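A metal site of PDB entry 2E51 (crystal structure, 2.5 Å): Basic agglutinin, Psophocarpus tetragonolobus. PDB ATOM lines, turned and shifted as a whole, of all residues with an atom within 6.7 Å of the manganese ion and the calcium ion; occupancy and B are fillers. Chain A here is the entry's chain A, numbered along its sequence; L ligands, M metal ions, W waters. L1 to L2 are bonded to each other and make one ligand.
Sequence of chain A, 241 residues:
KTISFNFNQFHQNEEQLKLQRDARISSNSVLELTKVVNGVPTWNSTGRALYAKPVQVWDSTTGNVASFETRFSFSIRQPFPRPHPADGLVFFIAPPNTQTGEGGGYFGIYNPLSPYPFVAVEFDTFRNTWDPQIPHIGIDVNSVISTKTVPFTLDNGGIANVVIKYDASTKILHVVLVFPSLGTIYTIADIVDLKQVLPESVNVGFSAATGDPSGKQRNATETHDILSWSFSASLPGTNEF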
ATOM      1  N   ASP A  87      -0.864  17.652   7.107  1.00  0.00           N
ATOM      2  CA  ASP A  87      -0.322  17.318   5.800  1.00  0.00           C
ATOM      3  C   ASP A  87       0.210  18.531   5.078  1.00  0.00           C
ATOM      4  O   ASP A  87       1.142  18.439   4.274  1.00  0.00           O
ATOM      5  CB  ASP A  87      -1.379  16.647   4.934  1.00  0.00           C
ATOM      6  CG  ASP A  87      -1.360  15.134   5.081  1.00  0.00           C
ATOM      7  OD1 ASP A  87      -2.170  14.614   5.865  1.00  0.00           O
ATOM      8  OD2 ASP A  87      -0.520  14.491   4.426  1.00  0.00           O
ATOM      9  N   GLY A 104      -6.015  14.339   3.843  1.00  0.00           N
ATOM     10  CA  GLY A 104      -4.655  13.851   3.768  1.00  0.00           C
ATOM     11  C   GLY A 104      -3.791  14.612   2.764  1.00  0.00           C
ATOM     12  O   GLY A 104      -3.889  15.847   2.652  1.00  0.00           O
ATOM     13  N   GLY A 105      -2.961  13.860   2.041  1.00  0.00           N
ATOM     14  CA  GLY A 105      -2.061  14.433   1.056  1.00  0.00           C
ATOM     15  C   GLY A 105      -2.769  15.079  -0.108  1.00  0.00           C
ATOM     16  O   GLY A 105      -2.114  15.595  -0.997  1.00  0.00           O
ATOM     17  N   TYR A 106      -4.102  15.039  -0.113  1.00  0.00           N
ATOM     18  CA  TYR A 106      -4.889  15.671  -1.184  1.00  0.00           C
ATOM     19  C   TYR A 106      -5.336  17.065  -0.763  1.00  0.00           C
ATOM     20  O   TYR A 106      -6.012  17.773  -1.518  1.00  0.00           O
ATOM     21  CB  TYR A 106      -6.076  14.797  -1.523  1.00  0.00           C
ATOM     22  CG  TYR A 106      -5.685  13.519  -2.237  1.00  0.00           C
ATOM     23  CD1 TYR A 106      -5.047  13.551  -3.465  1.00  0.00           C
ATOM     24  CD2 TYR A 106      -5.940  12.270  -1.656  1.00  0.00           C
ATOM     25  CE1 TYR A 106      -4.660  12.382  -4.128  1.00  0.00           C
ATOM     26  CE2 TYR A 106      -5.556  11.077  -2.304  1.00  0.00           C
ATOM     27  CZ  TYR A 106      -4.921  11.149  -3.549  1.00  0.00           C
ATOM     28  OH  TYR A 106      -4.552   9.990  -4.188  1.00  0.00           O
ATOM     29  N   PHE A 107      -4.937  17.456   0.450  1.00  0.00           N
ATOM     30  CA  PHE A 107      -5.216  18.781   0.997  1.00  0.00           C
ATOM     31  C   PHE A 107      -6.661  19.249   0.998  1.00  0.00           C
ATOM     32  O   PHE A 107      -6.944  20.370   1.396  1.00  0.00           O
ATOM     33  CB  PHE A 107      -4.371  19.825   0.249  1.00  0.00           C
ATOM     34  CG  PHE A 107      -2.906  19.455   0.102  1.00  0.00           C
ATOM     35  CD1 PHE A 107      -2.081  19.420   1.191  1.00  0.00           C
ATOM     36  CD2 PHE A 107      -2.369  19.205  -1.153  1.00  0.00           C
ATOM     37  CE1 PHE A 107      -0.705  19.150   1.049  1.00  0.00           C
ATOM     38  CE2 PHE A 107      -1.039  18.942  -1.305  1.00  0.00           C
ATOM     39  CZ  PHE A 107      -0.187  18.912  -0.204  1.00  0.00           C
ATOM     40  N   GLU A 122       1.240  24.688  -3.021  1.00  0.00           N
ATOM     41  CA  GLU A 122       1.224  23.945  -1.781  1.00  0.00           C
ATOM     42  C   GLU A 122       2.450  24.149  -0.881  1.00  0.00           C
ATOM     43  O   GLU A 122       3.553  24.445  -1.345  1.00  0.00           O
ATOM     44  CB  GLU A 122       1.119  22.463  -2.074  1.00  0.00           C
ATOM     45  CG  GLU A 122       2.347  21.931  -2.776  1.00  0.00           C
ATOM     46  CD  GLU A 122       2.322  20.420  -2.979  1.00  0.00           C
ATOM     47  OE1 GLU A 122       1.285  19.896  -3.465  1.00  0.00           O
ATOM     48  OE2 GLU A 122       3.345  19.790  -2.661  1.00  0.00           O
ATOM     49  N   ASP A 124       3.701  21.704   1.498  1.00  0.00           N
ATOM     50  CA  ASP A 124       3.575  20.323   1.860  1.00  0.00           C
ATOM     51  C   ASP A 124       4.480  19.897   2.988  1.00  0.00           C
ATOM     52  O   ASP A 124       5.697  20.052   2.897  1.00  0.00           O
ATOM     53  CB  ASP A 124       3.854  19.492   0.619  1.00  0.00           C
ATOM     54  CG  ASP A 124       3.361  18.086   0.732  1.00  0.00           C
ATOM     55  OD1 ASP A 124       3.006  17.655   1.846  1.00  0.00           O
ATOM     56  OD2 ASP A 124       3.344  17.409  -0.305  1.00  0.00           O
ATOM     57  N   THR A 125       3.903  19.310   4.035  1.00  0.00           N
ATOM     58  CA  THR A 125       4.705  18.907   5.176  1.00  0.00           C
ATOM     59  C   THR A 125       4.834  17.396   5.390  1.00  0.00           C
ATOM     60  O   THR A 125       5.567  16.955   6.272  1.00  0.00           O
ATOM     61  CB  THR A 125       4.150  19.526   6.435  1.00  0.00           C
ATOM     62  OG1 THR A 125       2.763  19.169   6.545  1.00  0.00           O
ATOM     63  CG2 THR A 125       4.276  21.038   6.384  1.00  0.00           C
ATOM     64  N   PHE A 126       4.126  16.595   4.604  1.00  0.00           N
ATOM     65  CA  PHE A 126       4.183  15.154   4.741  1.00  0.00           C
ATOM     66  C   PHE A 126       4.552  14.526   3.414  1.00  0.00           C
ATOM     67  O   PHE A 126       3.948  14.841   2.363  1.00  0.00           O
ATOM     68  CB  PHE A 126       2.851  14.591   5.200  1.00  0.00           C
ATOM     69  CG  PHE A 126       2.821  13.087   5.220  1.00  0.00           C
ATOM     70  CD1 PHE A 126       3.274  12.393   6.332  1.00  0.00           C
ATOM     71  CD2 PHE A 126       2.351  12.380   4.118  1.00  0.00           C
ATOM     72  CE1 PHE A 126       3.268  10.996   6.352  1.00  0.00           C
ATOM     73  CE2 PHE A 126       2.336  10.991   4.121  1.00  0.00           C
ATOM     74  CZ  PHE A 126       2.790  10.296   5.233  1.00  0.00           C
ATOM     75  N   ARG A 127       5.520  13.628   3.459  1.00  0.00           N
ATOM     76  CA  ARG A 127       5.968  12.984   2.230  1.00  0.00           C
ATOM     77  C   ARG A 127       5.164  11.777   1.780  1.00  0.00           C
ATOM     78  O   ARG A 127       5.325  10.716   2.322  1.00  0.00           O
ATOM     79  CB  ARG A 127       7.455  12.599   2.342  1.00  0.00           C
ATOM     80  CG  ARG A 127       7.973  12.021   1.058  1.00  0.00           C
ATOM     81  CD  ARG A 127       9.501  11.913   1.033  1.00  0.00           C
ATOM     82  NE  ARG A 127       9.958  11.469  -0.293  1.00  0.00           N
ATOM     83  CZ  ARG A 127      11.232  11.489  -0.676  1.00  0.00           C
ATOM     84  NH1 ARG A 127      12.170  11.929   0.135  1.00  0.00           N
ATOM     85  NH2 ARG A 127      11.553  11.068  -1.887  1.00  0.00           N
ATOM     86  N   ASN A 128       4.313  11.968   0.785  1.00  0.00           N
ATOM     87  CA  ASN A 128       3.530  10.865   0.240  1.00  0.00           C
ATOM     88  C   ASN A 128       4.381  10.125  -0.776  1.00  0.00           C
ATOM     89  O   ASN A 128       5.500  10.529  -1.069  1.00  0.00           O
ATOM     90  CB  ASN A 128       2.261  11.358  -0.426  1.00  0.00           C
ATOM     91  CG  ASN A 128       1.287  11.967   0.557  1.00  0.00           C
ATOM     92  OD1 ASN A 128       1.520  13.079   1.080  1.00  0.00           O
ATOM     93  ND2 ASN A 128       0.192  11.252   0.843  1.00  0.00           N
ATOM     94  N   TRP A 130       4.215  10.043  -3.890  1.00  0.00           N
ATOM     95  CA  TRP A 130       4.495  10.910  -5.038  1.00  0.00           C
ATOM     96  C   TRP A 130       5.324  12.162  -4.737  1.00  0.00           C
ATOM     97  O   TRP A 130       5.618  12.936  -5.645  1.00  0.00           O
ATOM     98  CB  TRP A 130       3.170  11.327  -5.661  1.00  0.00           C
ATOM     99  CG  TRP A 130       2.289  12.093  -4.703  1.00  0.00           C
ATOM    100  CD1 TRP A 130       2.459  13.394  -4.270  1.00  0.00           C
ATOM    101  CD2 TRP A 130       1.139  11.601  -4.014  1.00  0.00           C
ATOM    102  NE1 TRP A 130       1.497  13.718  -3.348  1.00  0.00           N
ATOM    103  CE2 TRP A 130       0.668  12.642  -3.174  1.00  0.00           C
ATOM    104  CE3 TRP A 130       0.452  10.380  -4.011  1.00  0.00           C
ATOM    105  CZ2 TRP A 130      -0.445  12.492  -2.351  1.00  0.00           C
ATOM    106  CZ3 TRP A 130      -0.667  10.222  -3.190  1.00  0.00           C
ATOM    107  CH2 TRP A 130      -1.097  11.272  -2.377  1.00  0.00           C
ATOM    108  N   ASP A 131       5.698  12.332  -3.466  1.00  0.00           N
ATOM    109  CA  ASP A 131       6.454  13.499  -3.010  1.00  0.00           C
ATOM    110  C   ASP A 131       7.945  13.404  -2.891  1.00  0.00           C
ATOM    111  O   ASP A 131       8.500  12.327  -2.648  1.00  0.00           O
ATOM    112  CB  ASP A 131       6.026  13.925  -1.575  1.00  0.00           C
ATOM    113  CG  ASP A 131       4.768  14.774  -1.535  1.00  0.00           C
ATOM    114  OD1 ASP A 131       4.526  15.514  -2.504  1.00  0.00           O
ATOM    115  OD2 ASP A 131       4.075  14.699  -0.490  1.00  0.00           O
ATOM    116  N   PRO A 132       8.628  14.557  -3.043  1.00  0.00           N
ATOM    117  CA  PRO A 132      10.088  14.643  -2.913  1.00  0.00           C
ATOM    118  C   PRO A 132      10.233  14.966  -1.423  1.00  0.00           C
ATOM    119  O   PRO A 132       9.246  15.045  -0.718  1.00  0.00           O
ATOM    120  CB  PRO A 132      10.457  15.829  -3.806  1.00  0.00           C
ATOM    121  CG  PRO A 132       9.248  16.690  -3.749  1.00  0.00           C
ATOM    122  CD  PRO A 132       8.116  15.660  -3.873  1.00  0.00           C
ATOM    123  N   ILE A 134      10.309  16.577   2.187  1.00  0.00           N
ATOM    124  CA  ILE A 134       9.488  17.644   2.756  1.00  0.00           C
ATOM    125  C   ILE A 134      10.244  18.356   3.875  1.00  0.00           C
ATOM    126  O   ILE A 134      11.160  17.803   4.448  1.00  0.00           O
ATOM    127  CB  ILE A 134       8.101  17.099   3.311  1.00  0.00           C
ATOM    128  CG1 ILE A 134       8.287  15.943   4.291  1.00  0.00           C
ATOM    129  CG2 ILE A 134       7.243  16.645   2.178  1.00  0.00           C
ATOM    130  CD1 ILE A 134       8.891  16.332   5.679  1.00  0.00           C
ATOM    131  N   HIS A 136       8.207  21.114   1.341  1.00  0.00           N
ATOM    132  CA  HIS A 136       8.515  21.703   0.056  1.00  0.00           C
ATOM    133  C   HIS A 136       7.389  22.595  -0.443  1.00  0.00           C
ATOM    134  O   HIS A 136       6.230  22.468  -0.044  1.00  0.00           O
ATOM    135  CB  HIS A 136       8.839  20.616  -1.009  1.00  0.00           C
ATOM    136  CG  HIS A 136       7.774  19.584  -1.227  1.00  0.00           C
ATOM    137  ND1 HIS A 136       7.866  18.295  -0.751  1.00  0.00           N
ATOM    138  CD2 HIS A 136       6.595  19.645  -1.900  1.00  0.00           C
ATOM    139  CE1 HIS A 136       6.811  17.602  -1.124  1.00  0.00           C
ATOM    140  NE2 HIS A 136       6.016  18.389  -1.821  1.00  0.00           N
ATOM    141  N   GLY A 138       5.349  23.690  -3.701  1.00  0.00           N
ATOM    142  CA  GLY A 138       5.070  23.022  -4.953  1.00  0.00           C
ATOM    143  C   GLY A 138       4.000  23.741  -5.749  1.00  0.00           C
ATOM    144  O   GLY A 138       3.123  24.369  -5.167  1.00  0.00           O
ATOM    145  N   ASP A 140       1.034  23.086  -8.244  1.00  0.00           N
ATOM    146  CA  ASP A 140       0.167  22.010  -8.700  1.00  0.00           C
ATOM    147  C   ASP A 140      -0.848  22.455  -9.729  1.00  0.00           C
ATOM    148  O   ASP A 140      -1.466  23.493  -9.585  1.00  0.00           O
ATOM    149  CB  ASP A 140      -0.583  21.373  -7.506  1.00  0.00           C
ATOM    150  CG  ASP A 140       0.361  20.803  -6.449  1.00  0.00           C
ATOM    151  OD1 ASP A 140       1.593  20.974  -6.552  1.00  0.00           O
ATOM    152  OD2 ASP A 140      -0.140  20.161  -5.512  1.00  0.00           O
ATOM    153  N   VAL A 144      -1.960  16.799  -7.424  1.00  0.00           N
ATOM    154  CA  VAL A 144      -1.070  17.124  -6.327  1.00  0.00           C
ATOM    155  C   VAL A 144       0.343  16.657  -6.624  1.00  0.00           C
ATOM    156  O   VAL A 144       1.215  16.723  -5.777  1.00  0.00           O
ATOM    157  CB  VAL A 144      -1.569  16.506  -5.008  1.00  0.00           C
ATOM    158  CG1 VAL A 144      -2.590  17.450  -4.358  1.00  0.00           C
ATOM    159  CG2 VAL A 144      -2.217  15.150  -5.301  1.00  0.00           C
ATOM    160  N   ILE A 145       0.557  16.152  -7.832  1.00  0.00           N
ATOM    161  CA  ILE A 145       1.900  15.732  -8.240  1.00  0.00           C
ATOM    162  C   ILE A 145       2.478  16.972  -8.926  1.00  0.00           C
ATOM    163  O   ILE A 145       2.288  17.193 -10.115  1.00  0.00           O
ATOM    164  CB  ILE A 145       1.832  14.572  -9.239  1.00  0.00           C
ATOM    165  CG1 ILE A 145       1.132  13.385  -8.590  1.00  0.00           C
ATOM    166  CG2 ILE A 145       3.215  14.150  -9.668  1.00  0.00           C
ATOM    167  CD1 ILE A 145       1.004  12.212  -9.528  1.00  0.00           C
ATOM    168  N   SER A 146       3.160  17.803  -8.126  1.00  0.00           N
ATOM    169  CA  SER A 146       3.710  19.086  -8.538  1.00  0.00           C
ATOM    170  C   SER A 146       4.505  19.110  -9.812  1.00  0.00           C
ATOM    171  O   SER A 146       5.271  18.202 -10.091  1.00  0.00           O
ATOM    172  CB  SER A 146       4.570  19.663  -7.411  1.00  0.00           C
ATOM    173  OG  SER A 146       3.855  19.660  -6.180  1.00  0.00           O
ATOM    174  N   THR A 149       8.930  21.795  -7.752  1.00  0.00           N
ATOM    175  CA  THR A 149       9.019  21.720  -6.303  1.00  0.00           C
ATOM    176  C   THR A 149      10.309  22.381  -5.784  1.00  0.00           C
ATOM    177  O   THR A 149      11.321  22.457  -6.494  1.00  0.00           O
ATOM    178  CB  THR A 149       8.988  20.205  -5.891  1.00  0.00           C
ATOM    179  OG1 THR A 149       7.630  19.791  -5.641  1.00  0.00           O
ATOM    180  CG2 THR A 149       9.839  19.945  -4.675  1.00  0.00           C
HETATM  181  C1  LIG L   1      -1.027   4.276   4.814  1.00  0.00           C
HETATM  182  C2  LIG L   1      -1.371   5.784   4.946  1.00  0.00           C
HETATM  183  C3  LIG L   1      -0.393   6.646   4.098  1.00  0.00           C
HETATM  184  C4  LIG L   1       1.041   6.309   4.486  1.00  0.00           C
HETATM  185  C5  LIG L   1       1.307   4.796   4.331  1.00  0.00           C
HETATM  186  C6  LIG L   1       2.723   4.430   4.774  1.00  0.00           C
HETATM  187  O1  LIG L   1      -1.262   3.838   3.522  1.00  0.00           O
HETATM  188  O2  LIG L   1      -2.710   6.020   4.526  1.00  0.00           O
HETATM  189  O3  LIG L   1      -0.594   8.088   4.250  1.00  0.00           O
HETATM  190  O4  LIG L   1       1.270   6.721   5.829  1.00  0.00           O
HETATM  191  O5  LIG L   1       0.360   4.026   5.144  1.00  0.00           O
HETATM  192  O6  LIG L   1       2.990   3.052   4.619  1.00  0.00           O
HETATM  193  O1  LG2 L   2      -1.584   8.996   6.226  1.00  0.00           O
HETATM  194  C1  LG2 L   2      -1.767   8.653   4.831  1.00  0.00           C
HETATM  195  C2  LG2 L   2      -2.194   9.916   4.018  1.00  0.00           C
HETATM  196  N1  LG2 L   2      -2.330   9.592   2.596  1.00  0.00           N
HETATM  197  C3  LG2 L   2      -1.126  11.030   4.247  1.00  0.00           C
HETATM  198  O2  LG2 L   2      -1.428  12.197   3.509  1.00  0.00           O
HETATM  199  C4  LG2 L   2      -0.990  11.334   5.757  1.00  0.00           C
HETATM  200  O3  LG2 L   2      -2.210  11.852   6.280  1.00  0.00           O
HETATM  201  C5  LG2 L   2      -0.615  10.041   6.510  1.00  0.00           C
HETATM  202  C6  LG2 L   2      -0.570  10.260   8.027  1.00  0.00           C
HETATM  203  O4  LG2 L   2      -0.199   9.096   8.743  1.00  0.00           O
HETATM  204  C7  LG2 L   2      -3.404   9.952   1.870  1.00  0.00           C
HETATM  205  O5  LG2 L   2      -4.352  10.617   2.313  1.00  0.00           O
HETATM  206  C8  LG2 L   2      -3.413   9.518   0.409  1.00  0.00           C
HETATM  207 MN    MN M   1       3.705  17.547  -2.538  1.00  0.00          MN
HETATM  208 CA    CA M   2       2.213  15.378   0.807  1.00  0.00          CA
HETATM  209  O   HOH W   1       0.610  15.739  -0.928  1.00  0.00           O
HETATM  210  O   HOH W   2       4.693  17.693  -4.610  1.00  0.00           O
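Of the 22 residues printed, 4 come within 4 Å of the manganese ion.
Within 4 Å of the calcium ion: Asp 124, Phe 126, Asn 128 and Asp 131.
The side-chain amide nitrogen of Asn 128 sits at hydrogen-bond distance from an oxygen (O2) of LG2 L2 (3.3 Å).
O2 of LG2 L2 is in hydrogen-bond range of N of Gly 105 (2.7 Å).
The side-chain carboxylate of Asp 87 sits at hydrogen-bond distance from an oxygen (O2) of LG2 L2, at 2.6 Å.
Water W1 lies within hydrogen-bond range of the backbone carbonyl oxygen (O) of Gly 105 (2.7 Å) and the indole nitrogen (NE1) of Trp 130 (3.3 Å).
The manganese ion is bound by OD1 of Asp 131, at 2.2 Å.
OD2 of Asp 124 binds the manganese ion.
The side-chain carboxylate (OE2) of Glu 122 binds the manganese ion (2.3 Å).
Water W2 binds the manganese ion (2.3 Å).
The manganese ion is bound by NE2 of His 136.
The manganese ion has five donor atoms within binding distance.
The guanidinium group (NE) of Arg 127 lies within hydrogen-bond range of the backbone carbonyl oxygen (O) of Asp 131 (2.9 Å).
The side-chain carboxylate of Glu 122 lies close to the side-chain carboxylate of Asp 140 (2.5 Å).
The backbone NH (N) of Glu 122 sits at hydrogen-bond distance from the backbone carbonyl oxygen (O) of Gly 138, 2.9 Å away.
OD2 of Asp 131 is bound to the calcium ion (2.4 Å).
Water W1 is bound to the calcium ion, at 2.4 Å.
The calcium ion is bound by O of Phe 126 (2.4 Å).
OD1 of Asn 128 is bound to the calcium ion.
The calcium ion is bound by OD2 of Asp 124, 2.6 Å away.
The calcium ion is bound by OD1 of Asp 124 (2.6 Å).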
